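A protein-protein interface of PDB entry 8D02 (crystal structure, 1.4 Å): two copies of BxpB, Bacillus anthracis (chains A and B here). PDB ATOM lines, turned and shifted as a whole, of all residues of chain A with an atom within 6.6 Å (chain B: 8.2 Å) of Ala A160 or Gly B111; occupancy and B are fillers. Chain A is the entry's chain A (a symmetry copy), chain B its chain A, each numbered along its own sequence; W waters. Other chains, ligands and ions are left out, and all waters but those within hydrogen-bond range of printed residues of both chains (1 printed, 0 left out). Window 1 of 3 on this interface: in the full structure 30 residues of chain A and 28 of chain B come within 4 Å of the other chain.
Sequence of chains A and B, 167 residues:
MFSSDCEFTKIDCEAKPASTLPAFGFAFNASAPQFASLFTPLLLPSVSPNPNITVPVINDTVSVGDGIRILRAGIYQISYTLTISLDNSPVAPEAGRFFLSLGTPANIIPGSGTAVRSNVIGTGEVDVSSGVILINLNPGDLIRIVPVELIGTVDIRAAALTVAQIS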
ATOM      1  N   PHE A  26      -7.199  -0.486 -22.379  1.00  0.00           N
ATOM      2  CA  PHE A  26      -6.759  -1.299 -21.248  1.00  0.00           C
ATOM      3  C   PHE A  26      -7.431  -2.640 -21.390  1.00  0.00           C
ATOM      4  O   PHE A  26      -8.660  -2.699 -21.453  1.00  0.00           O
ATOM      5  CB  PHE A  26      -7.135  -0.658 -19.911  1.00  0.00           C
ATOM      6  CG  PHE A  26      -6.644  -1.422 -18.704  1.00  0.00           C
ATOM      7  CD1 PHE A  26      -5.369  -1.989 -18.666  1.00  0.00           C
ATOM      8  CD2 PHE A  26      -7.461  -1.536 -17.581  1.00  0.00           C
ATOM      9  CE1 PHE A  26      -4.952  -2.668 -17.542  1.00  0.00           C
ATOM     10  CE2 PHE A  26      -7.017  -2.212 -16.447  1.00  0.00           C
ATOM     11  CZ  PHE A  26      -5.798  -2.787 -16.439  1.00  0.00           C
ATOM     12  N   ALA A  27      -6.650  -3.711 -21.423  1.00  0.00           N
ATOM     13  CA  ALA A  27      -7.174  -5.067 -21.507  1.00  0.00           C
ATOM     14  C   ALA A  27      -6.481  -5.913 -20.446  1.00  0.00           C
ATOM     15  O   ALA A  27      -5.260  -5.813 -20.264  1.00  0.00           O
ATOM     16  CB  ALA A  27      -6.996  -5.662 -22.902  1.00  0.00           C
ATOM     17  N   PHE A  28      -7.232  -6.745 -19.740  1.00  0.00           N
ATOM     18  CA  PHE A  28      -6.650  -7.524 -18.652  1.00  0.00           C
ATOM     19  C   PHE A  28      -7.344  -8.864 -18.492  1.00  0.00           C
ATOM     20  O   PHE A  28      -8.460  -9.103 -18.982  1.00  0.00           O
ATOM     21  CB  PHE A  28      -6.641  -6.706 -17.365  1.00  0.00           C
ATOM     22  CG  PHE A  28      -8.021  -6.331 -16.849  1.00  0.00           C
ATOM     23  CD1 PHE A  28      -8.642  -5.149 -17.266  1.00  0.00           C
ATOM     24  CD2 PHE A  28      -8.665  -7.121 -15.898  1.00  0.00           C
ATOM     25  CE1 PHE A  28      -9.898  -4.782 -16.749  1.00  0.00           C
ATOM     26  CE2 PHE A  28      -9.929  -6.734 -15.394  1.00  0.00           C
ATOM     27  CZ  PHE A  28     -10.519  -5.591 -15.849  1.00  0.00           C
ATOM     28  N   ASN A  29      -6.687  -9.699 -17.696  1.00  0.00           N
ATOM     29  CA  ASN A  29      -7.231 -10.981 -17.249  1.00  0.00           C
ATOM     30  C   ASN A  29      -7.001 -11.026 -15.754  1.00  0.00           C
ATOM     31  O   ASN A  29      -5.859 -11.144 -15.294  1.00  0.00           O
ATOM     32  CB  ASN A  29      -6.515 -12.132 -17.940  1.00  0.00           C
ATOM     33  CG  ASN A  29      -7.257 -13.410 -17.787  1.00  0.00           C
ATOM     34  OD1 ASN A  29      -8.008 -13.605 -16.817  1.00  0.00           O
ATOM     35  ND2 ASN A  29      -7.116 -14.273 -18.776  1.00  0.00           N
ATOM     36  N   ALA A  30      -8.074 -10.845 -15.005  1.00  0.00           N
ATOM     37  CA  ALA A  30      -7.986 -10.848 -13.550  1.00  0.00           C
ATOM     38  C   ALA A  30      -8.418 -12.161 -12.917  1.00  0.00           C
ATOM     39  O   ALA A  30      -7.984 -12.435 -11.788  1.00  0.00           O
ATOM     40  CB  ALA A  30      -8.793  -9.674 -12.947  1.00  0.00           C
ATOM     41  N   LEU A  44      -6.763 -11.785 -22.774  1.00  0.00           N
ATOM     42  CA  LEU A  44      -7.045 -10.547 -22.041  1.00  0.00           C
ATOM     43  C   LEU A  44      -8.508 -10.204 -22.288  1.00  0.00           C
ATOM     44  O   LEU A  44      -8.831  -9.353 -23.130  1.00  0.00           O
ATOM     45  CB  LEU A  44      -6.117  -9.402 -22.494  1.00  0.00           C
ATOM     46  CG  LEU A  44      -4.614  -9.640 -22.410  1.00  0.00           C
ATOM     47  CD1 LEU A  44      -3.867  -8.621 -23.217  1.00  0.00           C
ATOM     48  CD2 LEU A  44      -4.195  -9.592 -20.905  1.00  0.00           C
ATOM     49  N   PRO A  49     -12.234  -1.900 -15.594  1.00  0.00           N
ATOM     50  CA  PRO A  49     -11.654  -2.076 -14.251  1.00  0.00           C
ATOM     51  C   PRO A  49     -12.341  -1.346 -13.114  1.00  0.00           C
ATOM     52  O   PRO A  49     -12.174  -1.783 -11.961  1.00  0.00           O
ATOM     53  CB  PRO A  49     -10.245  -1.490 -14.417  1.00  0.00           C
ATOM     54  CG  PRO A  49     -10.413  -0.426 -15.445  1.00  0.00           C
ATOM     55  CD  PRO A  49     -11.439  -0.982 -16.430  1.00  0.00           C
ATOM     56  N   SER A  79       2.357  -0.636 -21.501  1.00  0.00           N
ATOM     57  CA  SER A  79       2.835  -1.393 -20.349  1.00  0.00           C
ATOM     58  C   SER A  79       2.197  -2.765 -20.363  1.00  0.00           C
ATOM     59  O   SER A  79       1.094  -2.956 -20.894  1.00  0.00           O
ATOM     60  CB  SER A  79       2.533  -0.647 -19.073  1.00  0.00           C
ATOM     61  OG  SER A  79       1.240  -0.970 -18.601  1.00  0.00           O
ATOM     62  N   TYR A  80       2.867  -3.725 -19.751  1.00  0.00           N
ATOM     63  CA  TYR A  80       2.222  -5.003 -19.442  1.00  0.00           C
ATOM     64  C   TYR A  80       2.684  -5.463 -18.080  1.00  0.00           C
ATOM     65  O   TYR A  80       3.810  -5.156 -17.673  1.00  0.00           O
ATOM     66  CB  TYR A  80       2.425  -6.063 -20.523  1.00  0.00           C
ATOM     67  CG  TYR A  80       3.822  -6.619 -20.698  1.00  0.00           C
ATOM     68  CD1 TYR A  80       4.789  -5.933 -21.455  1.00  0.00           C
ATOM     69  CD2 TYR A  80       4.154  -7.857 -20.174  1.00  0.00           C
ATOM     70  CE1 TYR A  80       6.051  -6.498 -21.652  1.00  0.00           C
ATOM     71  CE2 TYR A  80       5.419  -8.397 -20.346  1.00  0.00           C
ATOM     72  CZ  TYR A  80       6.339  -7.708 -21.108  1.00  0.00           C
ATOM     73  OH  TYR A  80       7.591  -8.285 -21.301  1.00  0.00           O
ATOM     74  N   THR A  81       1.824  -6.182 -17.380  1.00  0.00           N
ATOM     75  CA  THR A  81       2.065  -6.664 -16.010  1.00  0.00           C
ATOM     76  C   THR A  81       1.592  -8.103 -15.945  1.00  0.00           C
ATOM     77  O   THR A  81       0.477  -8.398 -16.368  1.00  0.00           O
ATOM     78  CB  THR A  81       1.275  -5.831 -14.965  1.00  0.00           C
ATOM     79  OG1 THR A  81       1.615  -4.439 -15.069  1.00  0.00           O
ATOM     80  CG2 THR A  81       1.591  -6.263 -13.592  1.00  0.00           C
ATOM     81  N   LEU A  82       2.414  -8.999 -15.421  1.00  0.00           N
ATOM     82  CA  LEU A  82       2.113 -10.418 -15.304  1.00  0.00           C
ATOM     83  C   LEU A  82       2.424 -10.901 -13.907  1.00  0.00           C
ATOM     84  O   LEU A  82       3.499 -10.587 -13.369  1.00  0.00           O
ATOM     85  CB  LEU A  82       2.994 -11.268 -16.269  1.00  0.00           C
ATOM     86  CG  LEU A  82       2.997 -10.832 -17.747  1.00  0.00           C
ATOM     87  CD1 LEU A  82       4.056 -11.601 -18.566  1.00  0.00           C
ATOM     88  CD2 LEU A  82       1.626 -11.055 -18.293  1.00  0.00           C
ATOM     89  N   ILE A 145       0.863  -9.723 -25.860  1.00  0.00           N
ATOM     90  CA  ILE A 145       1.927 -10.218 -24.978  1.00  0.00           C
ATOM     91  C   ILE A 145       2.202 -11.654 -25.374  1.00  0.00           C
ATOM     92  O   ILE A 145       1.298 -12.505 -25.326  1.00  0.00           O
ATOM     93  CB  ILE A 145       1.480 -10.171 -23.509  1.00  0.00           C
ATOM     94  CG1 ILE A 145       0.931  -8.793 -23.090  1.00  0.00           C
ATOM     95  CG2 ILE A 145       2.646 -10.572 -22.626  1.00  0.00           C
ATOM     96  CD1 ILE A 145       0.229  -8.820 -21.768  1.00  0.00           C
ATOM     97  N   ALA A 158      -2.363 -13.738 -13.654  1.00  0.00           N
ATOM     98  CA  ALA A 158      -3.056 -12.502 -14.024  1.00  0.00           C
ATOM     99  C   ALA A 158      -2.205 -11.796 -15.056  1.00  0.00           C
ATOM    100  O   ALA A 158      -0.981 -11.937 -15.053  1.00  0.00           O
ATOM    101  CB  ALA A 158      -3.185 -11.582 -12.813  1.00  0.00           C
ATOM    102  N   ALA A 159      -2.863 -11.058 -15.973  1.00  0.00           N
ATOM    103  CA  ALA A 159      -2.128 -10.326 -17.004  1.00  0.00           C
ATOM    104  C   ALA A 159      -2.840  -9.030 -17.284  1.00  0.00           C
ATOM    105  O   ALA A 159      -4.060  -8.953 -17.114  1.00  0.00           O
ATOM    106  CB  ALA A 159      -2.037 -11.133 -18.321  1.00  0.00           C
ATOM    107  N   ALA A 160      -2.108  -8.010 -17.699  1.00  0.00           N
ATOM    108  CA  ALA A 160      -2.705  -6.708 -18.004  1.00  0.00           C
ATOM    109  C   ALA A 160      -1.843  -6.021 -19.057  1.00  0.00           C
ATOM    110  O   ALA A 160      -0.635  -6.215 -19.082  1.00  0.00           O
ATOM    111  CB  ALA A 160      -2.835  -5.845 -16.754  1.00  0.00           C
ATOM    112  N   LEU A 161      -2.481  -5.200 -19.899  1.00  0.00           N
ATOM    113  CA  LEU A 161      -1.859  -4.510 -21.026  1.00  0.00           C
ATOM    114  C   LEU A 161      -2.485  -3.123 -21.114  1.00  0.00           C
ATOM    115  O   LEU A 161      -3.722  -3.003 -21.241  1.00  0.00           O
ATOM    116  CB  LEU A 161      -2.128  -5.280 -22.312  1.00  0.00           C
ATOM    117  CG  LEU A 161      -1.620  -4.616 -23.587  1.00  0.00           C
ATOM    118  CD1 LEU A 161      -0.077  -4.676 -23.649  1.00  0.00           C
ATOM    119  CD2 LEU A 161      -2.212  -5.360 -24.804  1.00  0.00           C
ATOM    120  N   THR A 162      -1.662  -2.075 -20.989  1.00  0.00           N
ATOM    121  CA  THR A 162      -2.119  -0.693 -21.167  1.00  0.00           C
ATOM    122  C   THR A 162      -1.482  -0.068 -22.392  1.00  0.00           C
ATOM    123  O   THR A 162      -0.317  -0.298 -22.696  1.00  0.00           O
ATOM    124  CB  THR A 162      -1.817   0.222 -19.981  1.00  0.00           C
ATOM    125  OG1 THR A 162      -0.416   0.511 -19.882  1.00  0.00           O
ATOM    126  CG2 THR A 162      -2.317  -0.317 -18.637  1.00  0.00           C
ATOM    127  N   ILE B  78      -2.524   4.770 -13.783  1.00  0.00           N
ATOM    128  CA  ILE B  78      -2.094   4.630 -12.401  1.00  0.00           C
ATOM    129  C   ILE B  78      -1.068   3.508 -12.355  1.00  0.00           C
ATOM    130  O   ILE B  78      -1.292   2.406 -12.897  1.00  0.00           O
ATOM    131  CB  ILE B  78      -3.281   4.391 -11.451  1.00  0.00           C
ATOM    132  CG1 ILE B  78      -4.276   5.566 -11.621  1.00  0.00           C
ATOM    133  CG2 ILE B  78      -2.796   4.181 -10.010  1.00  0.00           C
ATOM    134  CD1 ILE B  78      -5.502   5.510 -10.755  1.00  0.00           C
ATOM    135  N   TYR B  80       1.748   1.401  -9.549  1.00  0.00           N
ATOM    136  CA  TYR B  80       2.313   1.245  -8.207  1.00  0.00           C
ATOM    137  C   TYR B  80       3.505   0.321  -8.286  1.00  0.00           C
ATOM    138  O   TYR B  80       3.542  -0.567  -9.145  1.00  0.00           O
ATOM    139  CB  TYR B  80       1.289   0.798  -7.165  1.00  0.00           C
ATOM    140  CG  TYR B  80       0.746  -0.610  -7.282  1.00  0.00           C
ATOM    141  CD1 TYR B  80      -0.304  -0.914  -8.168  1.00  0.00           C
ATOM    142  CD2 TYR B  80       1.226  -1.616  -6.462  1.00  0.00           C
ATOM    143  CE1 TYR B  80      -0.827  -2.208  -8.212  1.00  0.00           C
ATOM    144  CE2 TYR B  80       0.723  -2.906  -6.533  1.00  0.00           C
ATOM    145  CZ  TYR B  80      -0.317  -3.168  -7.400  1.00  0.00           C
ATOM    146  OH  TYR B  80      -0.833  -4.461  -7.429  1.00  0.00           O
ATOM    147  N   PHE B  98      -1.779  -7.986  -3.790  1.00  0.00           N
ATOM    148  CA  PHE B  98      -2.038  -6.555  -3.670  1.00  0.00           C
ATOM    149  C   PHE B  98      -2.897  -6.084  -4.820  1.00  0.00           C
ATOM    150  O   PHE B  98      -2.826  -6.602  -5.939  1.00  0.00           O
ATOM    151  CB  PHE B  98      -0.737  -5.794  -3.681  1.00  0.00           C
ATOM    152  CG  PHE B  98       0.210  -6.239  -2.641  1.00  0.00           C
ATOM    153  CD1 PHE B  98       1.089  -7.281  -2.882  1.00  0.00           C
ATOM    154  CD2 PHE B  98       0.222  -5.628  -1.409  1.00  0.00           C
ATOM    155  CE1 PHE B  98       1.989  -7.695  -1.895  1.00  0.00           C
ATOM    156  CE2 PHE B  98       1.092  -6.074  -0.393  1.00  0.00           C
ATOM    157  CZ  PHE B  98       1.943  -7.115  -0.659  1.00  0.00           C
ATOM    158  N   PHE B  99      -3.749  -5.101  -4.532  1.00  0.00           N
ATOM    159  CA  PHE B  99      -4.541  -4.430  -5.559  1.00  0.00           C
ATOM    160  C   PHE B  99      -4.525  -2.929  -5.294  1.00  0.00           C
ATOM    161  O   PHE B  99      -4.235  -2.481  -4.180  1.00  0.00           O
ATOM    162  CB  PHE B  99      -6.020  -4.887  -5.474  1.00  0.00           C
ATOM    163  CG  PHE B  99      -6.295  -6.243  -6.083  1.00  0.00           C
ATOM    164  CD1 PHE B  99      -6.098  -7.392  -5.343  1.00  0.00           C
ATOM    165  CD2 PHE B  99      -6.806  -6.364  -7.352  1.00  0.00           C
ATOM    166  CE1 PHE B  99      -6.378  -8.636  -5.916  1.00  0.00           C
ATOM    167  CE2 PHE B  99      -7.096  -7.568  -7.915  1.00  0.00           C
ATOM    168  CZ  PHE B  99      -6.878  -8.715  -7.195  1.00  0.00           C
ATOM    169  N   LEU B 100      -4.878  -2.144  -6.310  1.00  0.00           N
ATOM    170  CA  LEU B 100      -5.348  -0.801  -6.036  1.00  0.00           C
ATOM    171  C   LEU B 100      -6.816  -0.878  -5.634  1.00  0.00           C
ATOM    172  O   LEU B 100      -7.562  -1.717  -6.133  1.00  0.00           O
ATOM    173  CB  LEU B 100      -5.205   0.007  -7.316  1.00  0.00           C
ATOM    174  CG  LEU B 100      -3.786   0.251  -7.772  1.00  0.00           C
ATOM    175  CD1 LEU B 100      -3.766   0.845  -9.183  1.00  0.00           C
ATOM    176  CD2 LEU B 100      -3.079   1.162  -6.774  1.00  0.00           C
ATOM    177  N   ILE B 108     -11.676  -3.333  -4.395  1.00  0.00           N
ATOM    178  CA  ILE B 108     -10.489  -3.483  -5.230  1.00  0.00           C
ATOM    179  C   ILE B 108     -10.811  -3.257  -6.701  1.00  0.00           C
ATOM    180  O   ILE B 108     -11.945  -3.441  -7.172  1.00  0.00           O
ATOM    181  CB  ILE B 108      -9.813  -4.834  -4.998  1.00  0.00           C
ATOM    182  CG1 ILE B 108     -10.741  -6.015  -5.336  1.00  0.00           C
ATOM    183  CG2 ILE B 108      -9.339  -4.890  -3.558  1.00  0.00           C
ATOM    184  CD1 ILE B 108     -10.006  -7.359  -5.293  1.00  0.00           C
ATOM    185  N   ILE B 109      -9.768  -2.914  -7.460  1.00  0.00           N
ATOM    186  CA  ILE B 109      -9.866  -2.632  -8.894  1.00  0.00           C
ATOM    187  C   ILE B 109      -9.382  -3.858  -9.671  1.00  0.00           C
ATOM    188  O   ILE B 109      -8.162  -4.101  -9.720  1.00  0.00           O
ATOM    189  CB  ILE B 109      -9.075  -1.374  -9.250  1.00  0.00           C
ATOM    190  CG1 ILE B 109      -9.722  -0.175  -8.544  1.00  0.00           C
ATOM    191  CG2 ILE B 109      -9.061  -1.133 -10.743  1.00  0.00           C
ATOM    192  CD1 ILE B 109      -8.834   1.071  -8.472  1.00  0.00           C
ATOM    193  N   PRO B 110     -10.281  -4.636 -10.312  1.00  0.00           N
ATOM    194  CA  PRO B 110      -9.808  -5.731 -11.179  1.00  0.00           C
ATOM    195  C   PRO B 110      -8.898  -5.180 -12.275  1.00  0.00           C
ATOM    196  O   PRO B 110      -9.152  -4.126 -12.861  1.00  0.00           O
ATOM    197  CB  PRO B 110     -11.101  -6.330 -11.753  1.00  0.00           C
ATOM    198  CG  PRO B 110     -12.176  -5.941 -10.780  1.00  0.00           C
ATOM    199  CD  PRO B 110     -11.755  -4.571 -10.273  1.00  0.00           C
ATOM    200  N   GLY B 111      -7.829  -5.904 -12.536  1.00  0.00           N
ATOM    201  CA  GLY B 111      -6.822  -5.493 -13.474  1.00  0.00           C
ATOM    202  C   GLY B 111      -5.583  -4.916 -12.814  1.00  0.00           C
ATOM    203  O   GLY B 111      -4.555  -4.760 -13.475  1.00  0.00           O
ATOM    204  N   SER B 112      -5.688  -4.568 -11.530  1.00  0.00           N
ATOM    205  CA  SER B 112      -4.577  -3.958 -10.789  1.00  0.00           C
ATOM    206  C   SER B 112      -3.862  -4.949  -9.886  1.00  0.00           C
ATOM    207  O   SER B 112      -2.958  -4.549  -9.145  1.00  0.00           O
ATOM    208  CB  SER B 112      -5.077  -2.765  -9.945  1.00  0.00           C
ATOM    209  OG  SER B 112      -5.819  -3.201  -8.805  1.00  0.00           O
ATOM    210  N   GLY B 113      -4.258  -6.210  -9.883  1.00  0.00           N
ATOM    211  CA  GLY B 113      -3.716  -7.176  -8.923  1.00  0.00           C
ATOM    212  C   GLY B 113      -2.311  -7.642  -9.282  1.00  0.00           C
ATOM    213  O   GLY B 113      -1.950  -7.795 -10.463  1.00  0.00           O
ATOM    214  N   THR B 114      -1.516  -7.862  -8.255  1.00  0.00           N
ATOM    215  CA  THR B 114      -0.207  -8.498  -8.383  1.00  0.00           C
ATOM    216  C   THR B 114      -0.032  -9.413  -7.183  1.00  0.00           C
ATOM    217  O   THR B 114      -0.677  -9.247  -6.147  1.00  0.00           O
ATOM    218  CB  THR B 114       0.941  -7.486  -8.430  1.00  0.00           C
ATOM    219  OG1 THR B 114       0.942  -6.675  -7.256  1.00  0.00           O
ATOM    220  CG2 THR B 114       0.911  -6.573  -9.684  1.00  0.00           C
ATOM    221  N   GLY B 131       2.692  -2.630 -11.109  1.00  0.00           N
ATOM    222  CA  GLY B 131       1.511  -2.793 -11.950  1.00  0.00           C
ATOM    223  C   GLY B 131       1.126  -1.444 -12.522  1.00  0.00           C
ATOM    224  O   GLY B 131       1.340  -0.416 -11.892  1.00  0.00           O
ATOM    225  N   VAL B 132       0.554  -1.449 -13.734  1.00  0.00           N
ATOM    226  CA  VAL B 132       0.003  -0.260 -14.402  1.00  0.00           C
ATOM    227  C   VAL B 132      -1.411  -0.569 -14.907  1.00  0.00           C
ATOM    228  O   VAL B 132      -1.666  -1.621 -15.527  1.00  0.00           O
ATOM    229  CB  VAL B 132       0.894   0.227 -15.568  1.00  0.00           C
ATOM    230  CG1 VAL B 132       0.420   1.592 -16.094  1.00  0.00           C
ATOM    231  CG2 VAL B 132       2.389   0.269 -15.169  1.00  0.00           C
ATOM    232  N   ILE B 133      -2.340   0.356 -14.665  1.00  0.00           N
ATOM    233  CA  ILE B 133      -3.706   0.293 -15.201  1.00  0.00           C
ATOM    234  C   ILE B 133      -4.074   1.627 -15.831  1.00  0.00           C
ATOM    235  O   ILE B 133      -3.407   2.648 -15.630  1.00  0.00           O
ATOM    236  CB  ILE B 133      -4.727  -0.074 -14.123  1.00  0.00           C
ATOM    237  CG1 ILE B 133      -4.964   1.067 -13.125  1.00  0.00           C
ATOM    238  CG2 ILE B 133      -4.316  -1.357 -13.387  1.00  0.00           C
ATOM    239  CD1 ILE B 133      -6.228   0.932 -12.296  1.00  0.00           C
ATOM    240  N   LEU B 134      -5.147   1.614 -16.615  1.00  0.00           N
ATOM    241  CA  LEU B 134      -5.906   2.808 -17.002  1.00  0.00           C
ATOM    242  C   LEU B 134      -7.306   2.695 -16.431  1.00  0.00           C
ATOM    243  O   LEU B 134      -7.877   1.591 -16.378  1.00  0.00           O
ATOM    244  CB  LEU B 134      -6.050   2.955 -18.514  1.00  0.00           C
ATOM    245  CG  LEU B 134      -4.799   3.082 -19.328  1.00  0.00           C
ATOM    246  CD1 LEU B 134      -5.070   2.997 -20.818  1.00  0.00           C
ATOM    247  CD2 LEU B 134      -4.089   4.383 -19.052  1.00  0.00           C
HETATM  248  O   HOH W   1       0.194  -3.089 -17.106  1.00  0.00           O
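N of Val B132 lies within hydrogen-bond range of OG1 of Thr A81 (3.4 Å).
The side-chain hydroxyl (OG) of Ser B112 lies within hydrogen-bond range of the backbone carbonyl oxygen (O) of Ile B109, at 2.7 Å. OH of Tyr B80 is in hydrogen-bond range of OG1 of Thr B114, 2.8 Å away. O of Leu B100 sits at hydrogen-bond distance from N of Ile B109 (2.8 Å). The backbone NH of Ile B133 lies within hydrogen-bond range of the backbone carbonyl oxygen of Ile B78 (2.9 Å). OG of Ser A79 is in hydrogen-bond range of OG1 of Thr A162 (2.6 Å). The backbone carbonyl oxygen (O) of Thr A81 lies within hydrogen-bond range of the backbone NH (N) of Ala A160 (2.9 Å).
Among the printed residues, pairs that only touch across the chains: Phe A26 with Gly B111 (3.8 Å), Phe A26 with Val B132 (3.99 Å), Phe A26 with Ile B133 (3.7 Å), Phe A26 with Leu B134 (3.4 Å), Phe A28 with Pro B110 (3.6 Å), Phe A28 with Gly B111 (3.5 Å), Ala A30 with Gly B111 (3.9 Å), Pro A49 with Ile B109 (3.4 Å), Pro A49 with Pro B110 (3.3 Å), Pro A49 with Leu B134 (3.4 Å), Ser A79 with Val B132 (3.3 Å), Thr A81 with Thr B114 (3.98 Å), Thr A81 with Gly B131 (3.5 Å), Ala A160 with Gly B111 (3.9 Å), Thr A162 with Val B132 (3.4 Å), Thr A162 with Ile B133 (3.8 Å) and Thr A162 with Leu B134 (3.98 Å).
Asn A29 touches none of the printed residues of chain B. Printed residues of chain B within 4 Å of Ala A30: Gly B111. Of the printed residues of chain B, Pro A49 touches Ile B109, Pro B110 and Leu B134. Leu A82 touches none of the printed residues of chain B. No residue of chain B comes within 4 Å of Ala A159. Of chain B, only Gly B111 comes within 4 Å of Ala A160. Printed residues of chain A within 4 Å of Ile B109: Pro A49. Printed residues of chain A within 4 Å of Gly B111: Phe A26, Phe A28, Ala A30 and Ala A160. The nearest residue of chain B that does not touch Ala A160 is Val B132 (4.6 Å).
Of the 16 printed residues of chain B, 8 touch a printed residue of chain A. Among the printed residues, 18 pairs touch across the chains. Among the printed residues, no Asp or Glu carboxylate lies within 4 Å of a Lys or Arg side-chain nitrogen of the other chain.
Position printed for both chains: 80. Of the 18 pairs that touch across the chains among the printed residues, none has its exchanged pair printed and touching as well.
Water W1 lies within hydrogen-bond range of the side-chain hydroxyl (OG) of Ser A79 (2.8 Å), the side-chain hydroxyl (OG1) of Thr A81 (2.8 Å) and the backbone carbonyl oxygen (O) of Val B132 (2.8 Å).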
